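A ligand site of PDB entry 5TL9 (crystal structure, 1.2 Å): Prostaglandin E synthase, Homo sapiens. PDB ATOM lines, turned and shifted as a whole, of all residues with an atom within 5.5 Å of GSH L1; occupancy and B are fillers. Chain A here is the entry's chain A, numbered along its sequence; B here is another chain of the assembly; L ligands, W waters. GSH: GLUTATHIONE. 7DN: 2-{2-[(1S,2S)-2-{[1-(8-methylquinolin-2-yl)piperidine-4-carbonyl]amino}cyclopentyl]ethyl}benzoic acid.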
ATOM      1  N   ARG A  72      16.349 -27.209   1.349  1.00  0.00           N
ATOM      2  CA  ARG A  72      14.913 -27.265   1.066  1.00  0.00           C
ATOM      3  C   ARG A  72      14.081 -26.668   2.191  1.00  0.00           C
ATOM      4  O   ARG A  72      13.133 -25.916   1.942  1.00  0.00           O
ATOM      5  CB  ARG A  72      14.435 -28.687   0.772  1.00  0.00           C
ATOM      6  CG  ARG A  72      14.925 -29.233  -0.554  1.00  0.00           C
ATOM      7  CD  ARG A  72      14.134 -30.454  -0.999  1.00  0.00           C
ATOM      8  NE  ARG A  72      14.315 -31.638  -0.142  1.00  0.00           N
ATOM      9  CZ  ARG A  72      15.352 -32.466  -0.201  1.00  0.00           C
ATOM     10  NH1 ARG A  72      16.350 -32.241  -1.054  1.00  0.00           N
ATOM     11  NH2 ARG A  72      15.399 -33.522   0.604  1.00  0.00           N
ATOM     12  N   ALA A  73      14.434 -26.986   3.439  1.00  0.00           N
ATOM     13  CA  ALA A  73      13.743 -26.426   4.594  1.00  0.00           C
ATOM     14  C   ALA A  73      13.902 -24.905   4.626  1.00  0.00           C
ATOM     15  O   ALA A  73      12.928 -24.177   4.840  1.00  0.00           O
ATOM     16  CB  ALA A  73      14.250 -27.056   5.880  1.00  0.00           C
ATOM     17  N   ARG A  75      14.637 -22.925   2.044  1.00  0.00           N
ATOM     18  CA  ARG A  75      13.885 -22.376   0.922  1.00  0.00           C
ATOM     19  C   ARG A  75      12.397 -22.309   1.238  1.00  0.00           C
ATOM     20  O   ARG A  75      11.742 -21.287   0.996  1.00  0.00           O
ATOM     21  CB  ARG A  75      14.155 -23.174  -0.358  1.00  0.00           C
ATOM     22  CG  ARG A  75      13.314 -22.729  -1.550  1.00  0.00           C
ATOM     23  CD  ARG A  75      13.462 -23.601  -2.810  1.00  0.00           C
ATOM     24  NE  ARG A  75      13.438 -25.066  -2.610  1.00  0.00           N
ATOM     25  CZ  ARG A  75      12.418 -25.788  -2.152  1.00  0.00           C
ATOM     26  NH1 ARG A  75      12.570 -27.101  -2.017  1.00  0.00           N
ATOM     27  NH2 ARG A  75      11.261 -25.223  -1.820  1.00  0.00           N
ATOM     28  N   ASN A  76      11.859 -23.386   1.800  1.00  0.00           N
ATOM     29  CA  ASN A  76      10.451 -23.392   2.156  1.00  0.00           C
ATOM     30  C   ASN A  76      10.108 -22.300   3.181  1.00  0.00           C
ATOM     31  O   ASN A  76       9.084 -21.624   3.060  1.00  0.00           O
ATOM     32  CB  ASN A  76      10.012 -24.779   2.619  1.00  0.00           C
ATOM     33  CG  ASN A  76       8.505 -24.906   2.694  1.00  0.00           C
ATOM     34  OD1 ASN A  76       7.896 -24.484   3.681  1.00  0.00           O
ATOM     35  ND2 ASN A  76       7.898 -25.477   1.655  1.00  0.00           N
ATOM     36  N   GLU A  79       9.786 -19.140   1.303  1.00  0.00           N
ATOM     37  CA  GLU A  79       8.511 -19.148   0.566  1.00  0.00           C
ATOM     38  C   GLU A  79       7.300 -18.791   1.436  1.00  0.00           C
ATOM     39  O   GLU A  79       6.249 -18.441   0.904  1.00  0.00           O
ATOM     40  CB  GLU A  79       8.307 -20.522  -0.107  1.00  0.00           C
ATOM     41  CG  GLU A  79       9.300 -20.798  -1.230  1.00  0.00           C
ATOM     42  CD  GLU A  79       9.296 -22.237  -1.754  1.00  0.00           C
ATOM     43  OE1 GLU A  79       8.485 -23.067  -1.302  1.00  0.00           O
ATOM     44  OE2 GLU A  79      10.122 -22.534  -2.642  1.00  0.00           O
ATOM     45  N   HIS A 115       7.072 -27.615  11.159  1.00  0.00           N
ATOM     46  CA  HIS A 115       7.511 -27.893   9.788  1.00  0.00           C
ATOM     47  C   HIS A 115       9.002 -28.180   9.715  1.00  0.00           C
ATOM     48  O   HIS A 115       9.427 -29.160   9.100  1.00  0.00           O
ATOM     49  CB  HIS A 115       7.131 -26.728   8.861  1.00  0.00           C
ATOM     50  CG  HIS A 115       7.419 -27.002   7.421  1.00  0.00           C
ATOM     51  ND1 HIS A 115       8.647 -26.725   6.843  1.00  0.00           N
ATOM     52  CD2 HIS A 115       6.657 -27.533   6.439  1.00  0.00           C
ATOM     53  CE1 HIS A 115       8.610 -27.071   5.567  1.00  0.00           C
ATOM     54  NE2 HIS A 115       7.414 -27.562   5.301  1.00  0.00           N
ATOM     55  N   TYR A 119      10.721 -31.644   8.781  1.00  0.00           N
ATOM     56  CA  TYR A 119      11.580 -31.679   7.588  1.00  0.00           C
ATOM     57  C   TYR A 119      12.969 -32.208   7.919  1.00  0.00           C
ATOM     58  O   TYR A 119      13.405 -33.206   7.344  1.00  0.00           O
ATOM     59  CB  TYR A 119      11.711 -30.288   6.923  1.00  0.00           C
ATOM     60  CG  TYR A 119      11.754 -30.347   5.406  1.00  0.00           C
ATOM     61  CD1 TYR A 119      12.089 -31.545   4.741  1.00  0.00           C
ATOM     62  CD2 TYR A 119      11.449 -29.231   4.623  1.00  0.00           C
ATOM     63  CE1 TYR A 119      12.104 -31.621   3.357  1.00  0.00           C
ATOM     64  CE2 TYR A 119      11.466 -29.302   3.231  1.00  0.00           C
ATOM     65  CZ  TYR A 119      11.787 -30.506   2.608  1.00  0.00           C
ATOM     66  OH  TYR A 119      11.789 -30.634   1.233  1.00  0.00           O
ATOM     67  N   ARG A 128       4.934 -33.358   7.727  1.00  0.00           N
ATOM     68  CA  ARG A 128       5.435 -32.072   7.230  1.00  0.00           C
ATOM     69  C   ARG A 128       4.387 -31.315   6.402  1.00  0.00           C
ATOM     70  O   ARG A 128       4.183 -30.119   6.608  1.00  0.00           O
ATOM     71  CB  ARG A 128       6.715 -32.258   6.409  1.00  0.00           C
ATOM     72  CG  ARG A 128       7.400 -30.948   6.046  1.00  0.00           C
ATOM     73  CD  ARG A 128       8.386 -31.127   4.904  1.00  0.00           C
ATOM     74  NE  ARG A 128       7.727 -31.318   3.612  1.00  0.00           N
ATOM     75  CZ  ARG A 128       7.656 -32.472   2.938  1.00  0.00           C
ATOM     76  NH1 ARG A 128       8.201 -33.597   3.406  1.00  0.00           N
ATOM     77  NH2 ARG A 128       7.027 -32.490   1.764  1.00  0.00           N
ATOM     78  N   SER A 129       3.733 -32.019   5.482  1.00  0.00           N
ATOM     79  CA  SER A 129       2.728 -31.404   4.612  1.00  0.00           C
ATOM     80  C   SER A 129       1.530 -30.856   5.384  1.00  0.00           C
ATOM     81  O   SER A 129       1.003 -29.786   5.043  1.00  0.00           O
ATOM     82  CB  SER A 129       2.265 -32.388   3.536  1.00  0.00           C
ATOM     83  OG  SER A 129       3.363 -32.804   2.735  1.00  0.00           O
ATOM     84  N   TYR A 132       2.694 -27.650   7.172  1.00  0.00           N
ATOM     85  CA  TYR A 132       2.748 -26.607   6.155  1.00  0.00           C
ATOM     86  C   TYR A 132       1.346 -26.019   5.926  1.00  0.00           C
ATOM     87  O   TYR A 132       1.164 -24.791   5.948  1.00  0.00           O
ATOM     88  CB  TYR A 132       3.293 -27.151   4.830  1.00  0.00           C
ATOM     89  CG  TYR A 132       3.382 -26.091   3.770  1.00  0.00           C
ATOM     90  CD1 TYR A 132       2.273 -25.754   2.978  1.00  0.00           C
ATOM     91  CD2 TYR A 132       4.569 -25.372   3.585  1.00  0.00           C
ATOM     92  CE1 TYR A 132       2.351 -24.742   2.032  1.00  0.00           C
ATOM     93  CE2 TYR A 132       4.662 -24.359   2.629  1.00  0.00           C
ATOM     94  CZ  TYR A 132       3.551 -24.047   1.857  1.00  0.00           C
ATOM     95  OH  TYR A 132       3.616 -23.048   0.923  1.00  0.00           O
ATOM     96  N   ALA B  33       2.998 -22.002  -5.364  1.00  0.00           N
ATOM     97  CA  ALA B  33       3.259 -23.090  -4.409  1.00  0.00           C
ATOM     98  C   ALA B  33       2.272 -24.246  -4.577  1.00  0.00           C
ATOM     99  O   ALA B  33       2.678 -25.426  -4.578  1.00  0.00           O
ATOM    100  CB  ALA B  33       3.243 -22.575  -2.975  1.00  0.00           C
ATOM    101  N   ILE B  34       0.987 -23.923  -4.732  1.00  0.00           N
ATOM    102  CA  ILE B  34      -0.065 -24.926  -4.892  1.00  0.00           C
ATOM    103  C   ILE B  34       0.089 -25.660  -6.227  1.00  0.00           C
ATOM    104  O   ILE B  34       0.013 -26.896  -6.263  1.00  0.00           O
ATOM    105  CB  ILE B  34      -1.463 -24.297  -4.718  1.00  0.00           C
ATOM    106  CG1 ILE B  34      -1.669 -23.871  -3.251  1.00  0.00           C
ATOM    107  CG2 ILE B  34      -2.569 -25.265  -5.152  1.00  0.00           C
ATOM    108  CD1 ILE B  34      -2.740 -22.831  -3.024  1.00  0.00           C
ATOM    109  N   THR B  36       2.881 -26.069  -7.844  1.00  0.00           N
ATOM    110  CA  THR B  36       4.071 -26.911  -7.668  1.00  0.00           C
ATOM    111  C   THR B  36       3.690 -28.264  -7.043  1.00  0.00           C
ATOM    112  O   THR B  36       4.101 -29.315  -7.549  1.00  0.00           O
ATOM    113  CB  THR B  36       5.148 -26.218  -6.799  1.00  0.00           C
ATOM    114  OG1 THR B  36       5.489 -24.950  -7.381  1.00  0.00           O
ATOM    115  CG2 THR B  36       6.394 -27.057  -6.708  1.00  0.00           C
ATOM    116  N   GLY B  37       2.902 -28.219  -5.977  1.00  0.00           N
ATOM    117  CA  GLY B  37       2.411 -29.437  -5.330  1.00  0.00           C
ATOM    118  C   GLY B  37       1.617 -30.338  -6.271  1.00  0.00           C
ATOM    119  O   GLY B  37       1.819 -31.556  -6.294  1.00  0.00           O
ATOM    120  N   ARG B  40       4.019 -32.007  -8.695  1.00  0.00           N
ATOM    121  CA  ARG B  40       4.695 -33.105  -7.992  1.00  0.00           C
ATOM    122  C   ARG B  40       3.824 -34.361  -7.918  1.00  0.00           C
ATOM    123  O   ARG B  40       4.294 -35.461  -8.209  1.00  0.00           O
ATOM    124  CB  ARG B  40       5.111 -32.694  -6.572  1.00  0.00           C
ATOM    125  CG  ARG B  40       6.245 -31.680  -6.511  1.00  0.00           C
ATOM    126  CD  ARG B  40       6.757 -31.568  -5.083  1.00  0.00           C
ATOM    127  NE  ARG B  40       7.889 -30.662  -4.949  1.00  0.00           N
ATOM    128  CZ  ARG B  40       9.146 -30.956  -5.290  1.00  0.00           C
ATOM    129  NH1 ARG B  40       9.463 -32.129  -5.842  1.00  0.00           N
ATOM    130  NH2 ARG B  40      10.102 -30.057  -5.101  1.00  0.00           N
ATOM    131  N   ALA B  47      10.587 -34.545  -3.707  1.00  0.00           N
ATOM    132  CA  ALA B  47      11.937 -34.135  -3.304  1.00  0.00           C
ATOM    133  C   ALA B  47      12.497 -34.992  -2.168  1.00  0.00           C
ATOM    134  O   ALA B  47      13.698 -34.991  -1.926  1.00  0.00           O
ATOM    135  CB  ALA B  47      11.937 -32.679  -2.917  1.00  0.00           C
ATOM    136  N   ASN B  48      11.606 -35.712  -1.480  1.00  0.00           N
ATOM    137  CA  ASN B  48      11.950 -36.409  -0.242  1.00  0.00           C
ATOM    138  C   ASN B  48      11.547 -37.862  -0.292  1.00  0.00           C
ATOM    139  O   ASN B  48      10.432 -38.165  -0.742  1.00  0.00           O
ATOM    140  CB  ASN B  48      11.260 -35.724   0.940  1.00  0.00           C
ATOM    141  CG  ASN B  48      11.572 -34.250   1.009  1.00  0.00           C
ATOM    142  OD1 ASN B  48      12.720 -33.862   1.215  1.00  0.00           O
ATOM    143  ND2 ASN B  48      10.557 -33.414   0.817  1.00  0.00           N
ATOM    144  N   ASP B  51       8.151 -38.638   1.272  1.00  0.00           N
ATOM    145  CA  ASP B  51       7.032 -38.276   0.408  1.00  0.00           C
ATOM    146  C   ASP B  51       6.790 -39.362  -0.629  1.00  0.00           C
ATOM    147  O   ASP B  51       5.661 -39.822  -0.807  1.00  0.00           O
ATOM    148  CB  ASP B  51       7.290 -36.937  -0.316  1.00  0.00           C
ATOM    149  CG  ASP B  51       7.501 -35.761   0.629  1.00  0.00           C
ATOM    150  OD1 ASP B  51       7.230 -35.854   1.849  1.00  0.00           O
ATOM    151  OD2 ASP B  51       7.955 -34.713   0.128  1.00  0.00           O
ATOM    152  N   VAL B  67       8.433 -29.634 -12.475  1.00  0.00           N
ATOM    153  CA  VAL B  67       8.623 -29.263 -11.073  1.00  0.00           C
ATOM    154  C   VAL B  67       9.749 -28.222 -10.956  1.00  0.00           C
ATOM    155  O   VAL B  67       9.574 -27.187 -10.309  1.00  0.00           O
ATOM    156  CB  VAL B  67       8.905 -30.492 -10.163  1.00  0.00           C
ATOM    157  CG1 VAL B  67       9.194 -30.038  -8.729  1.00  0.00           C
ATOM    158  CG2 VAL B  67       7.735 -31.460 -10.163  1.00  0.00           C
ATOM    159  N   LEU B  71       9.627 -24.330  -9.526  1.00  0.00           N
ATOM    160  CA  LEU B  71      10.555 -23.814  -8.530  1.00  0.00           C
ATOM    161  C   LEU B  71      11.308 -22.586  -9.037  1.00  0.00           C
ATOM    162  O   LEU B  71      11.531 -21.656  -8.264  1.00  0.00           O
ATOM    163  CB  LEU B  71      11.522 -24.906  -8.057  1.00  0.00           C
ATOM    164  CG  LEU B  71      10.904 -25.999  -7.176  1.00  0.00           C
ATOM    165  CD1 LEU B  71      11.797 -27.220  -7.122  1.00  0.00           C
ATOM    166  CD2 LEU B  71      10.623 -25.483  -5.774  1.00  0.00           C
ATOM    167  N   HIS B  74       8.913 -19.645  -8.811  1.00  0.00           N
ATOM    168  CA  HIS B  74       8.773 -19.290  -7.405  1.00  0.00           C
ATOM    169  C   HIS B  74      10.019 -18.567  -6.890  1.00  0.00           C
ATOM    170  O   HIS B  74       9.915 -17.558  -6.183  1.00  0.00           O
ATOM    171  CB  HIS B  74       8.483 -20.541  -6.576  1.00  0.00           C
ATOM    172  CG  HIS B  74       7.740 -20.269  -5.301  1.00  0.00           C
ATOM    173  ND1 HIS B  74       7.149 -21.270  -4.572  1.00  0.00           N
ATOM    174  CD2 HIS B  74       7.481 -19.111  -4.635  1.00  0.00           C
ATOM    175  CE1 HIS B  74       6.563 -20.752  -3.512  1.00  0.00           C
ATOM    176  NE2 HIS B  74       6.760 -19.442  -3.521  1.00  0.00           N
HETATM  177  N1  GSH L   1       8.386 -25.170  -3.192  1.00  0.00           N
HETATM  178  CA1 GSH L   1       7.424 -26.158  -2.624  1.00  0.00           C
HETATM  179  C1  GSH L   1       7.759 -27.562  -3.049  1.00  0.00           C
HETATM  180  O11 GSH L   1       7.185 -28.510  -2.479  1.00  0.00           O
HETATM  181  O12 GSH L   1       8.599 -27.752  -3.958  1.00  0.00           O
HETATM  182  CB1 GSH L   1       5.993 -25.736  -2.979  1.00  0.00           C
HETATM  183  CG1 GSH L   1       4.879 -26.481  -2.246  1.00  0.00           C
HETATM  184  CD1 GSH L   1       5.132 -26.629  -0.750  1.00  0.00           C
HETATM  185  OE1 GSH L   1       5.522 -25.680  -0.101  1.00  0.00           O
HETATM  186  N2  GSH L   1       4.901 -27.831  -0.208  1.00  0.00           N
HETATM  187  CA2 GSH L   1       5.136 -28.114   1.201  1.00  0.00           C
HETATM  188  C2  GSH L   1       6.560 -28.507   1.524  1.00  0.00           C
HETATM  189  O2  GSH L   1       6.872 -28.724   2.698  1.00  0.00           O
HETATM  190  CB2 GSH L   1       4.166 -29.191   1.679  1.00  0.00           C
HETATM  191  SG2 GSH L   1       4.331 -30.711   0.710  1.00  0.00           S
HETATM  192  N3  GSH L   1       7.415 -28.618   0.499  1.00  0.00           N
HETATM  193  CA3 GSH L   1       8.798 -29.071   0.634  1.00  0.00           C
HETATM  194  C3  GSH L   1       9.812 -28.136   0.027  1.00  0.00           C
HETATM  195  O31 GSH L   1       9.452 -26.981  -0.316  1.00  0.00           O
HETATM  196  O32 GSH L   1      10.978 -28.559  -0.090  1.00  0.00           O
HETATM  197  O1  7DN L   2      -0.244 -36.693   1.715  1.00  0.00           O
HETATM  198  C7  7DN L   2      -2.831 -24.766   1.801  1.00  0.00           C
HETATM  199  O2  7DN L   2      -2.416 -36.927   2.214  1.00  0.00           O
HETATM  200  C6  7DN L   2      -2.050 -25.853   1.389  1.00  0.00           C
HETATM  201  C1  7DN L   2       1.225 -28.915  -1.096  1.00  0.00           C
HETATM  202  N1  7DN L   2      -0.541 -24.372   0.308  1.00  0.00           N
HETATM  203  C5  7DN L   2      -0.889 -25.644   0.635  1.00  0.00           C
HETATM  204  C4  7DN L   2       0.913 -26.403  -0.888  1.00  0.00           C
HETATM  205  C3  7DN L   2       0.164 -27.883   0.973  1.00  0.00           C
HETATM  206  C2  7DN L   2       0.193 -29.093   0.032  1.00  0.00           C
HETATM  207  O   7DN L   2       0.274 -30.213  -2.902  1.00  0.00           O
HETATM  208  C15 7DN L   2       1.080 -30.127  -1.989  1.00  0.00           C
HETATM  209  N2  7DN L   2       1.956 -31.140  -1.642  1.00  0.00           N
HETATM  210  C16 7DN L   2       1.965 -32.430  -2.320  1.00  0.00           C
HETATM  211  C29 7DN L   2       3.252 -32.695  -3.108  1.00  0.00           C
HETATM  212  C28 7DN L   2       4.171 -33.469  -2.171  1.00  0.00           C
HETATM  213  C27 7DN L   2       3.313 -33.999  -1.030  1.00  0.00           C
HETATM  214  C17 7DN L   2       1.862 -33.602  -1.318  1.00  0.00           C
HETATM  215  C18 7DN L   2       1.108 -33.307  -0.029  1.00  0.00           C
HETATM  216  C19 7DN L   2      -0.223 -34.052   0.143  1.00  0.00           C
HETATM  217  C20 7DN L   2      -0.931 -33.740   1.443  1.00  0.00           C
HETATM  218  C21 7DN L   2      -1.097 -32.375   1.802  1.00  0.00           C
HETATM  219  C22 7DN L   2      -1.753 -31.994   2.988  1.00  0.00           C
HETATM  220  C23 7DN L   2      -2.256 -32.972   3.839  1.00  0.00           C
HETATM  221  C24 7DN L   2      -2.117 -34.332   3.514  1.00  0.00           C
HETATM  222  C25 7DN L   2      -1.454 -34.735   2.328  1.00  0.00           C
HETATM  223  C26 7DN L   2      -1.366 -36.232   2.081  1.00  0.00           C
HETATM  224  C   7DN L   2       1.031 -27.583  -1.850  1.00  0.00           C
HETATM  225  N   7DN L   2      -0.067 -26.666   0.191  1.00  0.00           N
HETATM  226  C8  7DN L   2      -2.464 -23.464   1.461  1.00  0.00           C
HETATM  227  C9  7DN L   2      -1.274 -23.292   0.688  1.00  0.00           C
HETATM  228  C13 7DN L   2      -3.219 -22.344   1.841  1.00  0.00           C
HETATM  229  C12 7DN L   2      -2.814 -21.058   1.473  1.00  0.00           C
HETATM  230  C11 7DN L   2      -1.649 -20.876   0.726  1.00  0.00           C
HETATM  231  C10 7DN L   2      -0.869 -21.988   0.333  1.00  0.00           C
HETATM  232  C14 7DN L   2       0.394 -21.783  -0.476  1.00  0.00           C
HETATM  233  O   HOH W   1       4.564 -29.753  -2.747  1.00  0.00           O
HETATM  234  O   HOH W   2       7.471 -23.889  -5.502  1.00  0.00           O
HETATM  235  O   HOH W   3       6.872 -31.153  -1.634  1.00  0.00           O
HETATM  236  O   HOH W   4       5.897 -22.967  -0.458  1.00  0.00           O
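A ring nitrogen (NE2) of His 115 lies within hydrogen-bond range of an oxygen (O2) of GSH L1, 2.9 Å away. NH1 of Arg 75 is in salt-bridge range of O32 of GSH L1 (2.9 Å). An oxygen (OE1) of GSH L1 lies close to the side-chain hydroxyl of Tyr 132 (3.4 Å). OH of Tyr 119 lies within hydrogen-bond range of O32 of GSH L1. ND2 of Asn 76 is in hydrogen-bond range of O31 of GSH L1 (2.9 Å). The side-chain carboxylate of Glu 79 lies within salt-bridge range of a nitrogen (N1) of GSH L1 (2.8 Å). An oxygen (O12) of GSH L1 is in salt-bridge range of the guanidinium group (NH2) of Arg 40 of chain B (3.0 Å). The side-chain hydroxyl of Ser 129 sits close to a sulfur (SG2) of GSH L1 (3.1 Å). The guanidinium group (NE) of Arg 128 lies within hydrogen-bond range of an oxygen (O2) of GSH L1 (2.9 Å).
NH2 of Arg 75 is in salt-bridge range of OE2 of Glu 79, at 3.0 Å. The side-chain amide nitrogen (ND2) of Asn 48 of chain B lies within hydrogen-bond range of the side-chain hydroxyl (OH) of Tyr 119 (3.1 Å). The guanidinium group (NH2) of Arg 72 lies within hydrogen-bond range of the backbone carbonyl oxygen (O) of Ala 47 of chain B (3.4 Å). NH1 of Arg 128 lies within salt-bridge range of OD1 of Asp 51 of chain B (2.9 Å). OH of Tyr 119 lies within hydrogen-bond range of NE of Arg 72 (3.0 Å). NH2 of Arg 72 lies within hydrogen-bond range of OD1 of Asn 48 of chain B (2.8 Å).
Water W4 lies within hydrogen-bond range of OH of Tyr 132 (2.7 Å), OE1 of Glu 79 (2.7 Å) and OE1 of GSH L1 (2.8 Å). Water W2 lies within hydrogen-bond range of N1 of GSH L1, ND1 of His 74 of chain B and OG1 of Thr 36 of chain B. Water W1 bridges O11 of GSH L1 and N2 of 7DN L2.
A sulfur (SG2) of GSH L1 sits close to a nitrogen (N2) of 7DN L2 (3.4 Å).
Residues that only touch GSH L1: Arg 72, Ala 33 of chain B, Thr 36 of chain B and Leu 71 of chain B. 13 residues have an atom within 4 Å of GSH L1: Arg 72, Arg 75, Asn 76, Glu 79, His 115, Tyr 119, Arg 128, Ser 129, Tyr 132, Ala 33 of chain B, Thr 36 of chain B, Arg 40 of chain B and Leu 71 of chain B. The nearest printed residue that does not touch GSH L1 is His 74 of chain B (4.3 Å).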
